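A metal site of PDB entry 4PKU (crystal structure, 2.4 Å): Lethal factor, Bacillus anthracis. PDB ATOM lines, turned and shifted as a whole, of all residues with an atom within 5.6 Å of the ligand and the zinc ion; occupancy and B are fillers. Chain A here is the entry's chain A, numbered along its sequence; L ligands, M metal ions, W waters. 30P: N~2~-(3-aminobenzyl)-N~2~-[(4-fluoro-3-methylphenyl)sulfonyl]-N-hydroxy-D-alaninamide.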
ATOM      1  N   ASP A  67      13.149  -6.454 -13.073  1.00  0.00           N
ATOM      2  CA  ASP A  67      13.627  -7.811 -13.333  1.00  0.00           C
ATOM      3  C   ASP A  67      13.041  -8.784 -12.313  1.00  0.00           C
ATOM      4  O   ASP A  67      13.298  -9.978 -12.354  1.00  0.00           O
ATOM      5  CB  ASP A  67      15.162  -7.870 -13.281  1.00  0.00           C
ATOM      6  CG  ASP A  67      15.812  -6.815 -14.160  1.00  0.00           C
ATOM      7  OD1 ASP A  67      15.246  -6.480 -15.212  1.00  0.00           O
ATOM      8  OD2 ASP A  67      16.896  -6.323 -13.775  1.00  0.00           O
ATOM      9  N   PHE A  68      12.245  -8.240 -11.407  1.00  0.00           N
ATOM     10  CA  PHE A  68      11.632  -9.023 -10.341  1.00  0.00           C
ATOM     11  C   PHE A  68      10.355  -9.701 -10.860  1.00  0.00           C
ATOM     12  O   PHE A  68       9.975 -10.776 -10.395  1.00  0.00           O
ATOM     13  CB  PHE A  68      11.339  -8.130  -9.126  1.00  0.00           C
ATOM     14  CG  PHE A  68      11.073  -8.883  -7.842  1.00  0.00           C
ATOM     15  CD1 PHE A  68      11.949  -8.773  -6.776  1.00  0.00           C
ATOM     16  CD2 PHE A  68       9.928  -9.643  -7.668  1.00  0.00           C
ATOM     17  CE1 PHE A  68      11.714  -9.447  -5.588  1.00  0.00           C
ATOM     18  CE2 PHE A  68       9.683 -10.318  -6.490  1.00  0.00           C
ATOM     19  CZ  PHE A  68      10.573 -10.216  -5.449  1.00  0.00           C
ATOM     20  N   VAL A 392      12.449 -16.554  -2.074  1.00  0.00           N
ATOM     21  CA  VAL A 392      13.004 -16.145  -3.353  1.00  0.00           C
ATOM     22  C   VAL A 392      12.957 -17.264  -4.393  1.00  0.00           C
ATOM     23  O   VAL A 392      13.352 -18.397  -4.099  1.00  0.00           O
ATOM     24  CB  VAL A 392      14.476 -15.671  -3.207  1.00  0.00           C
ATOM     25  CG1 VAL A 392      15.151 -15.547  -4.570  1.00  0.00           C
ATOM     26  CG2 VAL A 392      14.527 -14.359  -2.438  1.00  0.00           C
ATOM     27  N   HIS A 393      12.476 -16.949  -5.585  1.00  0.00           N
ATOM     28  CA  HIS A 393      12.734 -17.811  -6.735  1.00  0.00           C
ATOM     29  C   HIS A 393      13.649 -17.099  -7.711  1.00  0.00           C
ATOM     30  O   HIS A 393      13.446 -15.930  -8.039  1.00  0.00           O
ATOM     31  CB  HIS A 393      11.453 -18.223  -7.441  1.00  0.00           C
ATOM     32  CG  HIS A 393      11.698 -19.055  -8.665  1.00  0.00           C
ATOM     33  ND1 HIS A 393      12.450 -20.212  -8.629  1.00  0.00           N
ATOM     34  CD2 HIS A 393      11.324 -18.890  -9.954  1.00  0.00           C
ATOM     35  CE1 HIS A 393      12.517 -20.727  -9.837  1.00  0.00           C
ATOM     36  NE2 HIS A 393      11.838 -19.946 -10.666  1.00  0.00           N
ATOM     37  N   SER A 394      14.660 -17.818  -8.189  1.00  0.00           N
ATOM     38  CA  SER A 394      15.594 -17.281  -9.164  1.00  0.00           C
ATOM     39  C   SER A 394      16.448 -18.395  -9.745  1.00  0.00           C
ATOM     40  O   SER A 394      16.200 -19.577  -9.513  1.00  0.00           O
ATOM     41  CB  SER A 394      16.490 -16.218  -8.513  1.00  0.00           C
ATOM     42  OG  SER A 394      17.154 -16.732  -7.377  1.00  0.00           O
ATOM     43  N   LYS A 395      17.456 -18.007 -10.519  1.00  0.00           N
ATOM     44  CA  LYS A 395      18.377 -18.946 -11.132  1.00  0.00           C
ATOM     45  C   LYS A 395      19.168 -19.710 -10.071  1.00  0.00           C
ATOM     46  O   LYS A 395      19.233 -20.938 -10.088  1.00  0.00           O
ATOM     47  CB  LYS A 395      19.342 -18.226 -12.069  1.00  0.00           C
ATOM     48  CG  LYS A 395      20.266 -19.148 -12.834  1.00  0.00           C
ATOM     49  CD  LYS A 395      19.504 -19.860 -13.926  1.00  0.00           C
ATOM     50  CE  LYS A 395      20.105 -21.225 -14.213  1.00  0.00           C
ATOM     51  NZ  LYS A 395      19.287 -21.985 -15.196  1.00  0.00           N
ATOM     52  N   GLY A 396      19.739 -18.957  -9.143  1.00  0.00           N
ATOM     53  CA  GLY A 396      20.572 -19.536  -8.108  1.00  0.00           C
ATOM     54  C   GLY A 396      20.399 -18.849  -6.767  1.00  0.00           C
ATOM     55  O   GLY A 396      19.916 -17.712  -6.704  1.00  0.00           O
ATOM     56  N   LEU A 397      20.806 -19.526  -5.708  1.00  0.00           N
ATOM     57  CA  LEU A 397      20.668 -18.996  -4.362  1.00  0.00           C
ATOM     58  C   LEU A 397      21.697 -19.629  -3.429  1.00  0.00           C
ATOM     59  O   LEU A 397      22.043 -20.803  -3.589  1.00  0.00           O
ATOM     60  CB  LEU A 397      19.254 -19.248  -3.836  1.00  0.00           C
ATOM     61  CG  LEU A 397      18.704 -18.363  -2.718  1.00  0.00           C
ATOM     62  CD1 LEU A 397      18.734 -16.898  -3.127  1.00  0.00           C
ATOM     63  CD2 LEU A 397      17.289 -18.792  -2.346  1.00  0.00           C
ATOM     64  N   TYR A 398      22.195 -18.857  -2.477  1.00  0.00           N
ATOM     65  CA  TYR A 398      22.989 -19.424  -1.392  1.00  0.00           C
ATOM     66  C   TYR A 398      22.296 -19.147  -0.062  1.00  0.00           C
ATOM     67  O   TYR A 398      21.963 -18.005   0.246  1.00  0.00           O
ATOM     68  CB  TYR A 398      24.412 -18.860  -1.372  1.00  0.00           C
ATOM     69  CG  TYR A 398      25.220 -19.381  -0.203  1.00  0.00           C
ATOM     70  CD1 TYR A 398      25.718 -20.681  -0.198  1.00  0.00           C
ATOM     71  CD2 TYR A 398      25.469 -18.587   0.910  1.00  0.00           C
ATOM     72  CE1 TYR A 398      26.445 -21.167   0.865  1.00  0.00           C
ATOM     73  CE2 TYR A 398      26.203 -19.062   1.985  1.00  0.00           C
ATOM     74  CZ  TYR A 398      26.687 -20.356   1.952  1.00  0.00           C
ATOM     75  OH  TYR A 398      27.416 -20.844   3.025  1.00  0.00           O
ATOM     76  N   GLY A 413      18.718 -16.703 -15.760  1.00  0.00           N
ATOM     77  CA  GLY A 413      19.204 -15.700 -14.836  1.00  0.00           C
ATOM     78  C   GLY A 413      19.378 -14.369 -15.550  1.00  0.00           C
ATOM     79  O   GLY A 413      19.649 -14.343 -16.756  1.00  0.00           O
ATOM     80  N   VAL A 414      19.215 -13.269 -14.826  1.00  0.00           N
ATOM     81  CA  VAL A 414      19.345 -11.964 -15.447  1.00  0.00           C
ATOM     82  C   VAL A 414      20.820 -11.676 -15.762  1.00  0.00           C
ATOM     83  O   VAL A 414      21.692 -11.759 -14.906  1.00  0.00           O
ATOM     84  CB  VAL A 414      18.713 -10.832 -14.564  1.00  0.00           C
ATOM     85  CG1 VAL A 414      19.483 -10.626 -13.270  1.00  0.00           C
ATOM     86  CG2 VAL A 414      18.617  -9.531 -15.359  1.00  0.00           C
ATOM     87  N   GLU A 415      21.067 -11.388 -17.038  1.00  0.00           N
ATOM     88  CA  GLU A 415      22.411 -11.124 -17.552  1.00  0.00           C
ATOM     89  C   GLU A 415      23.423 -12.228 -17.208  1.00  0.00           C
ATOM     90  O   GLU A 415      24.581 -11.961 -16.905  1.00  0.00           O
ATOM     91  CB  GLU A 415      22.914  -9.775 -17.035  1.00  0.00           C
ATOM     92  CG  GLU A 415      22.130  -8.595 -17.594  1.00  0.00           C
ATOM     93  CD  GLU A 415      22.596  -7.261 -17.046  1.00  0.00           C
ATOM     94  OE1 GLU A 415      23.399  -7.260 -16.085  1.00  0.00           O
ATOM     95  OE2 GLU A 415      22.154  -6.220 -17.569  1.00  0.00           O
ATOM     96  N   LEU A 416      22.954 -13.477 -17.262  1.00  0.00           N
ATOM     97  CA  LEU A 416      23.820 -14.646 -17.180  1.00  0.00           C
ATOM     98  C   LEU A 416      23.855 -15.343 -18.530  1.00  0.00           C
ATOM     99  O   LEU A 416      22.832 -15.440 -19.208  1.00  0.00           O
ATOM    100  CB  LEU A 416      23.341 -15.616 -16.099  1.00  0.00           C
ATOM    101  CG  LEU A 416      23.753 -15.410 -14.648  1.00  0.00           C
ATOM    102  CD1 LEU A 416      23.089 -16.457 -13.775  1.00  0.00           C
ATOM    103  CD2 LEU A 416      25.264 -15.465 -14.498  1.00  0.00           C
ATOM    104  N   GLU A 421      28.188 -20.049 -14.979  1.00  0.00           N
ATOM    105  CA  GLU A 421      28.460 -18.719 -14.462  1.00  0.00           C
ATOM    106  C   GLU A 421      27.558 -18.436 -13.282  1.00  0.00           C
ATOM    107  O   GLU A 421      27.963 -17.830 -12.293  1.00  0.00           O
ATOM    108  CB  GLU A 421      28.289 -17.650 -15.543  1.00  0.00           C
ATOM    109  CG  GLU A 421      29.197 -17.843 -16.750  1.00  0.00           C
ATOM    110  CD  GLU A 421      29.161 -16.658 -17.699  1.00  0.00           C
ATOM    111  OE1 GLU A 421      28.105 -15.988 -17.783  1.00  0.00           O
ATOM    112  OE2 GLU A 421      30.199 -16.390 -18.343  1.00  0.00           O
ATOM    113  N   GLY A 422      26.309 -18.897 -13.388  1.00  0.00           N
ATOM    114  CA  GLY A 422      25.358 -18.782 -12.313  1.00  0.00           C
ATOM    115  C   GLY A 422      25.770 -19.523 -11.054  1.00  0.00           C
ATOM    116  O   GLY A 422      25.554 -19.040  -9.941  1.00  0.00           O
ATOM    117  N   HIS A 425      28.756 -17.677  -9.125  1.00  0.00           N
ATOM    118  CA  HIS A 425      28.287 -16.522  -8.380  1.00  0.00           C
ATOM    119  C   HIS A 425      27.802 -16.939  -6.986  1.00  0.00           C
ATOM    120  O   HIS A 425      28.123 -16.290  -5.995  1.00  0.00           O
ATOM    121  CB  HIS A 425      27.188 -15.801  -9.155  1.00  0.00           C
ATOM    122  CG  HIS A 425      26.349 -14.873  -8.335  1.00  0.00           C
ATOM    123  ND1 HIS A 425      26.520 -13.512  -8.351  1.00  0.00           N
ATOM    124  CD2 HIS A 425      25.304 -15.124  -7.508  1.00  0.00           C
ATOM    125  CE1 HIS A 425      25.631 -12.952  -7.545  1.00  0.00           C
ATOM    126  NE2 HIS A 425      24.884 -13.907  -7.023  1.00  0.00           N
ATOM    127  N   GLU A 426      27.033 -18.020  -6.936  1.00  0.00           N
ATOM    128  CA  GLU A 426      26.530 -18.551  -5.666  1.00  0.00           C
ATOM    129  C   GLU A 426      27.684 -19.043  -4.791  1.00  0.00           C
ATOM    130  O   GLU A 426      27.648 -18.907  -3.568  1.00  0.00           O
ATOM    131  CB  GLU A 426      25.550 -19.696  -5.902  1.00  0.00           C
ATOM    132  CG  GLU A 426      24.240 -19.323  -6.582  1.00  0.00           C
ATOM    133  CD  GLU A 426      23.642 -18.016  -6.082  1.00  0.00           C
ATOM    134  OE1 GLU A 426      23.655 -17.766  -4.864  1.00  0.00           O
ATOM    135  OE2 GLU A 426      23.141 -17.246  -6.926  1.00  0.00           O
ATOM    136  N   HIS A 429      29.231 -16.442  -2.773  1.00  0.00           N
ATOM    137  CA  HIS A 429      28.540 -16.197  -1.514  1.00  0.00           C
ATOM    138  C   HIS A 429      29.080 -17.112  -0.423  1.00  0.00           C
ATOM    139  O   HIS A 429      29.281 -16.689   0.717  1.00  0.00           O
ATOM    140  CB  HIS A 429      27.039 -16.423  -1.660  1.00  0.00           C
ATOM    141  CG  HIS A 429      26.348 -15.333  -2.412  1.00  0.00           C
ATOM    142  ND1 HIS A 429      26.530 -13.996  -2.132  1.00  0.00           N
ATOM    143  CD2 HIS A 429      25.458 -15.386  -3.429  1.00  0.00           C
ATOM    144  CE1 HIS A 429      25.787 -13.270  -2.948  1.00  0.00           C
ATOM    145  NE2 HIS A 429      25.135 -14.088  -3.748  1.00  0.00           N
ATOM    146  N   TYR A 467      23.810  -5.465 -11.680  1.00  0.00           N
ATOM    147  CA  TYR A 467      23.251  -6.171 -10.536  1.00  0.00           C
ATOM    148  C   TYR A 467      24.199  -6.126  -9.351  1.00  0.00           C
ATOM    149  O   TYR A 467      23.766  -6.181  -8.196  1.00  0.00           O
ATOM    150  CB  TYR A 467      22.948  -7.630 -10.909  1.00  0.00           C
ATOM    151  CG  TYR A 467      22.392  -8.421  -9.747  1.00  0.00           C
ATOM    152  CD1 TYR A 467      21.281  -7.979  -9.042  1.00  0.00           C
ATOM    153  CD2 TYR A 467      22.987  -9.617  -9.348  1.00  0.00           C
ATOM    154  CE1 TYR A 467      20.779  -8.691  -7.980  1.00  0.00           C
ATOM    155  CE2 TYR A 467      22.480 -10.342  -8.289  1.00  0.00           C
ATOM    156  CZ  TYR A 467      21.376  -9.866  -7.607  1.00  0.00           C
ATOM    157  OH  TYR A 467      20.878 -10.587  -6.547  1.00  0.00           O
ATOM    158  N   GLU A 474      26.161  -8.957  -3.112  1.00  0.00           N
ATOM    159  CA  GLU A 474      26.001  -9.142  -4.546  1.00  0.00           C
ATOM    160  C   GLU A 474      27.228  -8.681  -5.325  1.00  0.00           C
ATOM    161  O   GLU A 474      27.643  -9.326  -6.277  1.00  0.00           O
ATOM    162  CB  GLU A 474      24.754  -8.407  -5.038  1.00  0.00           C
ATOM    163  CG  GLU A 474      23.456  -8.881  -4.411  1.00  0.00           C
ATOM    164  CD  GLU A 474      23.292 -10.388  -4.531  1.00  0.00           C
ATOM    165  OE1 GLU A 474      23.719 -10.933  -5.560  1.00  0.00           O
ATOM    166  OE2 GLU A 474      22.728 -11.003  -3.601  1.00  0.00           O
ATOM    167  N   ALA A 477      29.956 -11.318  -4.904  1.00  0.00           N
ATOM    168  CA  ALA A 477      29.675 -12.525  -5.669  1.00  0.00           C
ATOM    169  C   ALA A 477      29.836 -12.290  -7.169  1.00  0.00           C
ATOM    170  O   ALA A 477      30.330 -13.146  -7.896  1.00  0.00           O
ATOM    171  CB  ALA A 477      28.284 -13.035  -5.364  1.00  0.00           C
ATOM    172  N   GLU A 478      29.403 -11.116  -7.635  1.00  0.00           N
ATOM    173  CA  GLU A 478      29.527 -10.767  -9.047  1.00  0.00           C
ATOM    174  C   GLU A 478      30.975 -10.596  -9.454  1.00  0.00           C
ATOM    175  O   GLU A 478      31.384 -11.048 -10.517  1.00  0.00           O
ATOM    176  CB  GLU A 478      28.736  -9.493  -9.349  1.00  0.00           C
ATOM    177  CG  GLU A 478      27.240  -9.706  -9.523  1.00  0.00           C
ATOM    178  CD  GLU A 478      26.920 -10.564 -10.740  1.00  0.00           C
ATOM    179  OE1 GLU A 478      26.604  -9.997 -11.798  1.00  0.00           O
ATOM    180  OE2 GLU A 478      26.970 -11.808 -10.624  1.00  0.00           O
ATOM    181  N   ARG A 481      32.576 -14.009  -9.544  1.00  0.00           N
ATOM    182  CA  ARG A 481      32.178 -14.708 -10.759  1.00  0.00           C
ATOM    183  C   ARG A 481      32.967 -14.211 -11.968  1.00  0.00           C
ATOM    184  O   ARG A 481      33.513 -15.012 -12.727  1.00  0.00           O
ATOM    185  CB  ARG A 481      30.671 -14.537 -11.013  1.00  0.00           C
ATOM    186  CG  ARG A 481      30.248 -14.973 -12.402  1.00  0.00           C
ATOM    187  CD  ARG A 481      28.747 -14.815 -12.608  1.00  0.00           C
ATOM    188  NE  ARG A 481      28.329 -13.422 -12.722  1.00  0.00           N
ATOM    189  CZ  ARG A 481      28.396 -12.707 -13.836  1.00  0.00           C
ATOM    190  NH1 ARG A 481      28.880 -13.259 -14.947  1.00  0.00           N
ATOM    191  NH2 ARG A 481      28.000 -11.442 -13.842  1.00  0.00           N
HETATM  192  C21 30P L   1      15.681 -12.163  -9.622  1.00  0.00           C
HETATM  193  C20 30P L   1      16.916 -12.641  -9.202  1.00  0.00           C
HETATM  194  C22 30P L   1      15.573 -10.885 -10.160  1.00  0.00           C
HETATM  195  C23 30P L   1      16.700 -10.086 -10.269  1.00  0.00           C
HETATM  196  C24 30P L   1      17.936 -10.566  -9.840  1.00  0.00           C
HETATM  197  C19 30P L   1      18.057 -11.847  -9.314  1.00  0.00           C
HETATM  198  C18 30P L   1      19.416 -12.311  -8.843  1.00  0.00           C
HETATM  199  N6  30P L   1      19.573 -13.756  -8.702  1.00  0.00           N
HETATM  200  C1  30P L   1      19.571 -14.289  -7.335  1.00  0.00           C
HETATM  201  C28 30P L   1      18.575 -13.555  -6.436  1.00  0.00           C
HETATM  202  C2  30P L   1      20.908 -14.238  -6.664  1.00  0.00           C
HETATM  203  N4  30P L   1      21.421 -15.345  -6.126  1.00  0.00           N
HETATM  204  O5  30P L   1      22.438 -15.208  -5.268  1.00  0.00           O
HETATM  205  O3  30P L   1      21.711 -13.034  -6.527  1.00  0.00           O
HETATM  206  S7  30P L   1      19.786 -14.666  -9.902  1.00  0.00           S
HETATM  207  O8  30P L   1      18.987 -14.191 -10.991  1.00  0.00           O
HETATM  208  O9  30P L   1      19.409 -16.005  -9.563  1.00  0.00           O
HETATM  209  C10 30P L   1      21.325 -14.657 -10.322  1.00  0.00           C
HETATM  210  C15 30P L   1      22.139 -15.731  -9.978  1.00  0.00           C
HETATM  211  C14 30P L   1      23.479 -15.739 -10.328  1.00  0.00           C
HETATM  212  C13 30P L   1      24.022 -14.663 -11.031  1.00  0.00           C
HETATM  213  F16 30P L   1      25.316 -14.666 -11.385  1.00  0.00           F
HETATM  214  C12 30P L   1      23.211 -13.598 -11.379  1.00  0.00           C
HETATM  215  C11 30P L   1      21.872 -13.592 -11.019  1.00  0.00           C
HETATM  216  C17 30P L   1      23.791 -12.431 -12.135  1.00  0.00           C
HETATM  217  N1  30P L   1      14.457 -13.017  -9.507  1.00  0.00           N
HETATM  218 ZN    ZN M   1      23.297 -13.316  -5.216  1.00  0.00          ZN
HETATM  219  O   HOH W   1      21.565 -13.485  -3.082  1.00  0.00           O
HETATM  220  O   HOH W   2      21.925 -15.919  -2.814  1.00  0.00           O
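The zinc ion is bound by O3 of the ligand (2.1 Å), O5 of the ligand (2.1 Å), OE1 of Glu 474 (2.4 Å), NE2 of His 429 (2.5 Å) and NE2 of His 425 (2.5 Å).
The zinc ion has five donor atoms within binding distance.
Slightly farther from the zinc ion lies water W1 (2.8 Å).
The side-chain carboxylate (OE2) of Glu 478 lies close to a fluorine (F16) of the ligand (3.4 Å).
Asp 67 touches the ligand.
O of Val 414 touches C17 of the ligand, 3.5 Å away.
CD2 of Leu 416 touches F16 of the ligand, 3.2 Å away.
Gly 422 touches the ligand (O to C14, 3.9 Å).
Arg 481 touches the ligand.
Hydrophobic or aromatic side chains that line the ligand: Val 414, Leu 416, His 425, His 429 and Tyr 467.
Within 4 Å of the ligand: Asp 67, His 393, Ser 394, Lys 395, Gly 396, Val 414, Leu 416, Gly 422, His 425, Glu 426, His 429, Tyr 467, Glu 474, Glu 478 and Arg 481.
Along chain A the residues within 4 Å of the ligand span positions 67 to 481.
Merely in contact with the zinc ion: Tyr 467 (3.9 Å).
Four residues have an atom within 4 Å of the zinc ion: His 425, His 429, Tyr 467 and Glu 474.
The nearest printed residue that does not touch the zinc ion is Glu 426 (4.3 Å).
OH of Tyr 467 lies close to O3 of the ligand (2.6 Å).
OE2 of Glu 426 sits at hydrogen-bond distance from N4 of the ligand, 2.7 Å away.
The backbone NH (N) of Gly 396 lies within hydrogen-bond range of an oxygen (O9) of the ligand (3.0 Å).
The backbone carbonyl oxygen (O) of Gly 396 sits at hydrogen-bond distance from a nitrogen (N4) of the ligand (2.9 Å).
O9 of the ligand lies within hydrogen-bond range of N of Lys 395, 3.0 Å away.
The side-chain hydroxyl (OG) of Ser 394 sits close to an oxygen (O9) of the ligand (3.2 Å).
A nitrogen (N1) of the ligand sits at hydrogen-bond distance from the backbone carbonyl oxygen of His 393, at 3.4 Å.
The side-chain hydroxyl (OH) of Tyr 467 lies close to the side-chain carboxylate (OE1) of Glu 474, at 3.0 Å.
A ring nitrogen (ND1) of His 425 is in hydrogen-bond range of the side-chain carboxylate (OE2) of Glu 478 (2.9 Å).
The side-chain carboxylate (OE1) of Glu 426 lies close to the backbone NH (N) of Leu 397 (3.5 Å).
N of Tyr 398 lies within hydrogen-bond range of OE1 of Glu 426 (3.0 Å).
O of Gly 396 is in hydrogen-bond range of OG of Ser 394, 3.0 Å away.
The side-chain carboxylate of Glu 478 is in salt-bridge range of the guanidinium group of Arg 481, at 2.9 Å.
Water W2 lies within hydrogen-bond range of the backbone NH (N) of Tyr 398 (3.0 Å), the side-chain carboxylate (OE1) of Glu 426 (3.3 Å) and a nitrogen (N4) of the ligand (3.4 Å).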
